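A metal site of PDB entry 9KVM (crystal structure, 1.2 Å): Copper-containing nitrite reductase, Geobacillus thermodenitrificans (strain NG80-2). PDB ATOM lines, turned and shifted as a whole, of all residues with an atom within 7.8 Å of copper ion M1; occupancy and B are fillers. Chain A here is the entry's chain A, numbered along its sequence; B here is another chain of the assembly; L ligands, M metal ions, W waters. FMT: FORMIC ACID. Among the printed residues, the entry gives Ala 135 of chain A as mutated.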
ATOM      1  N   ASP A  98     -28.347  14.029  18.045  1.00  0.00           N
ATOM      2  CA  ASP A  98     -27.566  14.302  19.243  1.00  0.00           C
ATOM      3  C   ASP A  98     -26.382  15.137  18.792  1.00  0.00           C
ATOM      4  O   ASP A  98     -25.580  14.684  17.970  1.00  0.00           O
ATOM      5  CB  ASP A  98     -27.119  12.940  19.820  1.00  0.00           C
ATOM      6  CG  ASP A  98     -26.074  13.033  20.939  1.00  0.00           C
ATOM      7  OD1 ASP A  98     -25.410  14.073  21.123  1.00  0.00           O
ATOM      8  OD2 ASP A  98     -25.885  11.995  21.627  1.00  0.00           O
ATOM      9  N   PHE A  99     -26.279  16.367  19.277  1.00  0.00           N
ATOM     10  CA  PHE A  99     -25.115  17.215  19.036  1.00  0.00           C
ATOM     11  C   PHE A  99     -24.221  17.167  20.285  1.00  0.00           C
ATOM     12  O   PHE A  99     -24.674  17.516  21.377  1.00  0.00           O
ATOM     13  CB  PHE A  99     -25.506  18.685  18.854  1.00  0.00           C
ATOM     14  CG  PHE A  99     -26.194  19.018  17.545  1.00  0.00           C
ATOM     15  CD1 PHE A  99     -25.506  19.091  16.351  1.00  0.00           C
ATOM     16  CD2 PHE A  99     -27.537  19.343  17.542  1.00  0.00           C
ATOM     17  CE1 PHE A  99     -26.160  19.445  15.174  1.00  0.00           C
ATOM     18  CE2 PHE A  99     -28.198  19.691  16.382  1.00  0.00           C
ATOM     19  CZ  PHE A  99     -27.509  19.739  15.192  1.00  0.00           C
ATOM     20  N   HIS A 100     -22.953  16.789  20.130  1.00  0.00           N
ATOM     21  CA  HIS A 100     -22.055  16.813  21.294  1.00  0.00           C
ATOM     22  C   HIS A 100     -21.767  18.223  21.764  1.00  0.00           C
ATOM     23  O   HIS A 100     -21.247  18.400  22.868  1.00  0.00           O
ATOM     24  CB  HIS A 100     -20.724  16.142  20.968  1.00  0.00           C
ATOM     25  CG  HIS A 100     -20.776  14.649  20.970  1.00  0.00           C
ATOM     26  ND1 HIS A 100     -19.620  13.894  20.987  1.00  0.00           N
ATOM     27  CD2 HIS A 100     -21.795  13.762  20.980  1.00  0.00           C
ATOM     28  CE1 HIS A 100     -19.938  12.603  21.020  1.00  0.00           C
ATOM     29  NE2 HIS A 100     -21.254  12.506  21.023  1.00  0.00           N
ATOM     30  N   PHE A 110     -33.236  14.886  22.471  1.00  0.00           N
ATOM     31  CA  PHE A 110     -32.606  14.036  21.456  1.00  0.00           C
ATOM     32  C   PHE A 110     -33.536  12.871  21.098  1.00  0.00           C
ATOM     33  O   PHE A 110     -33.095  11.742  20.881  1.00  0.00           O
ATOM     34  CB  PHE A 110     -31.264  13.479  21.937  1.00  0.00           C
ATOM     35  CG  PHE A 110     -30.174  14.507  22.215  1.00  0.00           C
ATOM     36  CD1 PHE A 110     -30.246  15.827  21.805  1.00  0.00           C
ATOM     37  CD2 PHE A 110     -29.024  14.094  22.879  1.00  0.00           C
ATOM     38  CE1 PHE A 110     -29.175  16.713  22.059  1.00  0.00           C
ATOM     39  CE2 PHE A 110     -28.008  14.964  23.153  1.00  0.00           C
ATOM     40  CZ  PHE A 110     -28.054  16.258  22.732  1.00  0.00           C
ATOM     41  N   MET A 132     -18.652  16.104  17.491  1.00  0.00           N
ATOM     42  CA  MET A 132     -19.425  15.153  16.716  1.00  0.00           C
ATOM     43  C   MET A 132     -20.917  15.395  16.888  1.00  0.00           C
ATOM     44  O   MET A 132     -21.388  15.795  17.957  1.00  0.00           O
ATOM     45  CB  MET A 132     -19.085  13.739  17.179  1.00  0.00           C
ATOM     46  CG  MET A 132     -19.815  12.674  16.402  1.00  0.00           C
ATOM     47  SD  MET A 132     -19.264  11.015  16.911  1.00  0.00           S
ATOM     48  CE  MET A 132     -20.307   9.953  15.910  1.00  0.00           C
ATOM     49  N   TYR A 133     -21.675  15.119  15.831  1.00  0.00           N
ATOM     50  CA  TYR A 133     -23.111  14.925  15.947  1.00  0.00           C
ATOM     51  C   TYR A 133     -23.459  13.570  15.351  1.00  0.00           C
ATOM     52  O   TYR A 133     -22.730  13.039  14.519  1.00  0.00           O
ATOM     53  CB  TYR A 133     -23.929  16.096  15.358  1.00  0.00           C
ATOM     54  CG  TYR A 133     -23.963  16.254  13.854  1.00  0.00           C
ATOM     55  CD1 TYR A 133     -24.645  15.366  13.034  1.00  0.00           C
ATOM     56  CD2 TYR A 133     -23.342  17.355  13.247  1.00  0.00           C
ATOM     57  CE1 TYR A 133     -24.696  15.552  11.657  1.00  0.00           C
ATOM     58  CE2 TYR A 133     -23.408  17.550  11.858  1.00  0.00           C
ATOM     59  CZ  TYR A 133     -24.086  16.648  11.089  1.00  0.00           C
ATOM     60  OH  TYR A 133     -24.176  16.801   9.732  1.00  0.00           O
ATOM     61  N   HIS A 134     -24.587  13.000  15.782  1.00  0.00           N
ATOM     62  CA  HIS A 134     -24.997  11.703  15.274  1.00  0.00           C
ATOM     63  C   HIS A 134     -26.426  11.427  15.711  1.00  0.00           C
ATOM     64  O   HIS A 134     -26.950  12.087  16.597  1.00  0.00           O
ATOM     65  CB  HIS A 134     -24.041  10.573  15.760  1.00  0.00           C
ATOM     66  CG  HIS A 134     -23.950  10.439  17.248  1.00  0.00           C
ATOM     67  ND1 HIS A 134     -24.868   9.747  18.004  1.00  0.00           N
ATOM     68  CD2 HIS A 134     -23.019  10.908  18.122  1.00  0.00           C
ATOM     69  CE1 HIS A 134     -24.522   9.805  19.282  1.00  0.00           C
ATOM     70  NE2 HIS A 134     -23.404  10.500  19.374  1.00  0.00           N
ATOM     71  N   ALA A 135     -27.023  10.410  15.112  1.00  0.00           N
ATOM     72  CA  ALA A 135     -28.335   9.979  15.537  1.00  0.00           C
ATOM     73  C   ALA A 135     -28.253   9.326  16.916  1.00  0.00           C
ATOM     74  O   ALA A 135     -27.263   8.696  17.265  1.00  0.00           O
ATOM     75  CB  ALA A 135     -28.946   8.987  14.548  1.00  0.00           C
ATOM     76  N   GLY A 136     -29.306   9.519  17.701  1.00  0.00           N
ATOM     77  CA  GLY A 136     -29.407   8.993  19.048  1.00  0.00           C
ATOM     78  C   GLY A 136     -30.416   7.874  19.182  1.00  0.00           C
ATOM     79  O   GLY A 136     -30.740   7.495  20.309  1.00  0.00           O
ATOM     80  N   VAL A 140     -27.925   2.837  18.750  1.00  0.00           N
ATOM     81  CA  VAL A 140     -27.121   3.952  18.237  1.00  0.00           C
ATOM     82  C   VAL A 140     -26.018   3.448  17.304  1.00  0.00           C
ATOM     83  O   VAL A 140     -25.757   4.046  16.265  1.00  0.00           O
ATOM     84  CB  VAL A 140     -26.585   4.803  19.407  1.00  0.00           C
ATOM     85  CG1 VAL A 140     -25.639   5.894  18.904  1.00  0.00           C
ATOM     86  CG2 VAL A 140     -27.734   5.407  20.179  1.00  0.00           C
ATOM     87  N   ILE A 144     -25.126   5.081  13.598  1.00  0.00           N
ATOM     88  CA  ILE A 144     -23.819   5.668  13.283  1.00  0.00           C
ATOM     89  C   ILE A 144     -23.148   4.890  12.163  1.00  0.00           C
ATOM     90  O   ILE A 144     -22.675   5.475  11.185  1.00  0.00           O
ATOM     91  CB  ILE A 144     -22.908   5.762  14.511  1.00  0.00           C
ATOM     92  CG1 ILE A 144     -23.523   6.681  15.589  1.00  0.00           C
ATOM     93  CG2 ILE A 144     -21.547   6.308  14.077  1.00  0.00           C
ATOM     94  CD1 ILE A 144     -22.736   6.680  16.906  1.00  0.00           C
ATOM     95  N   ALA A 273     -12.734   7.791  19.733  1.00  0.00           N
ATOM     96  CA  ALA A 273     -13.940   7.790  18.914  1.00  0.00           C
ATOM     97  C   ALA A 273     -14.834   8.927  19.407  1.00  0.00           C
ATOM     98  O   ALA A 273     -15.137   8.991  20.598  1.00  0.00           O
ATOM     99  CB  ALA A 273     -14.647   6.447  19.067  1.00  0.00           C
ATOM    100  N   SER A 274     -15.216   9.817  18.473  1.00  0.00           N
ATOM    101  CA  SER A 274     -15.940  11.089  18.639  1.00  0.00           C
ATOM    102  C   SER A 274     -15.016  12.256  18.973  1.00  0.00           C
ATOM    103  O   SER A 274     -15.498  13.369  19.103  1.00  0.00           O
ATOM    104  CB  SER A 274     -17.107  11.090  19.639  1.00  0.00           C
ATOM    105  OG  SER A 274     -16.699  11.014  20.994  1.00  0.00           O
ATOM    106  N   HIS B 244     -17.707   9.365  27.445  1.00  0.00           N
ATOM    107  CA  HIS B 244     -18.562  10.481  27.070  1.00  0.00           C
ATOM    108  C   HIS B 244     -19.861  10.422  27.867  1.00  0.00           C
ATOM    109  O   HIS B 244     -20.431   9.342  28.028  1.00  0.00           O
ATOM    110  CB  HIS B 244     -18.880  10.365  25.556  1.00  0.00           C
ATOM    111  CG  HIS B 244     -19.847  11.372  25.046  1.00  0.00           C
ATOM    112  ND1 HIS B 244     -19.509  12.695  24.831  1.00  0.00           N
ATOM    113  CD2 HIS B 244     -21.158  11.269  24.713  1.00  0.00           C
ATOM    114  CE1 HIS B 244     -20.559  13.361  24.371  1.00  0.00           C
ATOM    115  NE2 HIS B 244     -21.574  12.522  24.300  1.00  0.00           N
ATOM    116  N   VAL B 245     -20.367  11.581  28.284  1.00  0.00           N
ATOM    117  CA  VAL B 245     -21.696  11.700  28.887  1.00  0.00           C
ATOM    118  C   VAL B 245     -22.584  12.424  27.901  1.00  0.00           C
ATOM    119  O   VAL B 245     -22.250  13.533  27.462  1.00  0.00           O
ATOM    120  CB  VAL B 245     -21.642  12.413  30.247  1.00  0.00           C
ATOM    121  CG1 VAL B 245     -23.048  12.545  30.826  1.00  0.00           C
ATOM    122  CG2 VAL B 245     -20.755  11.651  31.218  1.00  0.00           C
ATOM    123  N   VAL B 246     -23.684  11.797  27.503  1.00  0.00           N
ATOM    124  CA  VAL B 246     -24.577  12.367  26.507  1.00  0.00           C
ATOM    125  C   VAL B 246     -25.299  13.558  27.115  1.00  0.00           C
ATOM    126  O   VAL B 246     -25.754  13.519  28.259  1.00  0.00           O
ATOM    127  CB  VAL B 246     -25.563  11.279  26.043  1.00  0.00           C
ATOM    128  CG1 VAL B 246     -26.572  11.824  25.029  1.00  0.00           C
ATOM    129  CG2 VAL B 246     -24.808  10.051  25.467  1.00  0.00           C
ATOM    130  N   GLY B 247     -25.438  14.640  26.327  1.00  0.00           N
ATOM    131  CA  GLY B 247     -26.176  15.816  26.733  1.00  0.00           C
ATOM    132  C   GLY B 247     -25.400  16.857  27.508  1.00  0.00           C
ATOM    133  O   GLY B 247     -25.984  17.846  27.971  1.00  0.00           O
ATOM    134  N   GLN B 267     -15.376  16.922  24.937  1.00  0.00           N
ATOM    135  CA  GLN B 267     -16.589  16.130  24.698  1.00  0.00           C
ATOM    136  C   GLN B 267     -16.404  14.702  25.145  1.00  0.00           C
ATOM    137  O   GLN B 267     -17.348  14.073  25.633  1.00  0.00           O
ATOM    138  CB  GLN B 267     -17.003  16.151  23.220  1.00  0.00           C
ATOM    139  CG  GLN B 267     -16.114  15.389  22.241  1.00  0.00           C
ATOM    140  CD  GLN B 267     -16.397  15.823  20.823  1.00  0.00           C
ATOM    141  OE1 GLN B 267     -17.515  15.634  20.305  1.00  0.00           O
ATOM    142  NE2 GLN B 267     -15.409  16.451  20.183  1.00  0.00           N
ATOM    143  N   THR B 268     -15.175  14.186  25.016  1.00  0.00           N
ATOM    144  CA  THR B 268     -14.879  12.774  25.184  1.00  0.00           C
ATOM    145  C   THR B 268     -13.453  12.658  25.694  1.00  0.00           C
ATOM    146  O   THR B 268     -12.573  13.386  25.229  1.00  0.00           O
ATOM    147  CB  THR B 268     -15.029  12.048  23.840  1.00  0.00           C
ATOM    148  OG1 THR B 268     -16.407  12.141  23.474  1.00  0.00           O
ATOM    149  CG2 THR B 268     -14.612  10.578  23.908  1.00  0.00           C
ATOM    150  N   VAL B 292     -21.468   6.609  28.287  1.00  0.00           N
ATOM    151  CA  VAL B 292     -21.028   5.593  27.335  1.00  0.00           C
ATOM    152  C   VAL B 292     -19.524   5.612  27.182  1.00  0.00           C
ATOM    153  O   VAL B 292     -18.847   6.589  27.494  1.00  0.00           O
ATOM    154  CB  VAL B 292     -21.679   5.783  25.943  1.00  0.00           C
ATOM    155  CG1 VAL B 292     -23.184   5.839  26.033  1.00  0.00           C
ATOM    156  CG2 VAL B 292     -21.158   7.030  25.207  1.00  0.00           C
ATOM    157  N   HIS B 294     -17.720   5.781  23.702  1.00  0.00           N
ATOM    158  CA  HIS B 294     -18.155   6.154  22.365  1.00  0.00           C
ATOM    159  C   HIS B 294     -17.588   5.250  21.286  1.00  0.00           C
ATOM    160  O   HIS B 294     -17.906   5.456  20.111  1.00  0.00           O
ATOM    161  CB  HIS B 294     -17.873   7.629  22.082  1.00  0.00           C
ATOM    162  CG  HIS B 294     -19.000   8.326  21.381  1.00  0.00           C
ATOM    163  ND1 HIS B 294     -19.308   8.151  20.063  1.00  0.00           N
ATOM    164  CD2 HIS B 294     -19.928   9.182  21.863  1.00  0.00           C
ATOM    165  CE1 HIS B 294     -20.377   8.878  19.753  1.00  0.00           C
ATOM    166  NE2 HIS B 294     -20.771   9.508  20.843  1.00  0.00           N
ATOM    167  N   PHE B 296     -18.593   2.447  19.826  1.00  0.00           N
ATOM    168  CA  PHE B 296     -19.979   2.057  20.014  1.00  0.00           C
ATOM    169  C   PHE B 296     -20.221   0.561  19.923  1.00  0.00           C
ATOM    170  O   PHE B 296     -21.248   0.088  20.426  1.00  0.00           O
ATOM    171  CB  PHE B 296     -20.940   2.873  19.124  1.00  0.00           C
ATOM    172  CG  PHE B 296     -21.792   3.782  19.956  1.00  0.00           C
ATOM    173  CD1 PHE B 296     -22.926   3.305  20.586  1.00  0.00           C
ATOM    174  CD2 PHE B 296     -21.394   5.075  20.211  1.00  0.00           C
ATOM    175  CE1 PHE B 296     -23.676   4.121  21.433  1.00  0.00           C
ATOM    176  CE2 PHE B 296     -22.146   5.906  21.051  1.00  0.00           C
ATOM    177  CZ  PHE B 296     -23.271   5.420  21.670  1.00  0.00           C
HETATM  178  C   FMT L   1     -24.109   8.364  22.712  1.00  0.00           C
HETATM  179  O1  FMT L   1     -23.100   9.030  22.496  1.00  0.00           O
HETATM  180  O2  FMT L   1     -25.185   8.638  22.205  1.00  0.00           O
HETATM  181 CU    CU M   1     -22.297  10.775  21.096  1.00  0.00          CU
HETATM  182 CU    CU M   2     -22.884  13.354  23.625  1.00  0.00          CU
HETATM  183  O   HOH W   1     -23.577  11.225  22.383  1.00  0.00           O
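Copper ion M1 is bound by water W1 (1.9 Å), a ring nitrogen (NE2) of His 294 of chain B (2.0 Å), a ring nitrogen (NE2) of His 100 (2.0 Å), a ring nitrogen (NE2) of His 134 (2.1 Å) and an oxygen (O1) of the ligand (2.4 Å).
OD2 of Asp 98 touches copper ion M1, 3.8 Å away.
NE2 of His 244 of chain B touches copper ion M1 (3.7 Å).
Of the 22 residues printed, 5 come within 4 Å of copper ion M1.
The nearest printed residue that does not touch copper ion M1 is Phe 296 of chain B (4.9 Å).
ND1 of His 100 lies within hydrogen-bond range of OE1 of Gln 267 of chain B (2.8 Å).
The backbone carbonyl oxygen of His 244 of chain B sits at hydrogen-bond distance from the backbone NH of Val 292 of chain B (2.9 Å).
The backbone carbonyl oxygen of His 134 lies within hydrogen-bond range of the backbone NH of Asp 98 (2.8 Å).
A ring nitrogen (ND1) of His 244 of chain B sits at hydrogen-bond distance from the side-chain hydroxyl (OG1) of Thr 268 of chain B (3.4 Å).
The backbone carbonyl oxygen (O) of Gln 267 of chain B lies within hydrogen-bond range of a ring nitrogen (ND1) of His 244 of chain B (2.7 Å).
The backbone carbonyl oxygen (O) of Met 132 sits at hydrogen-bond distance from the backbone NH (N) of His 100 (2.9 Å).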
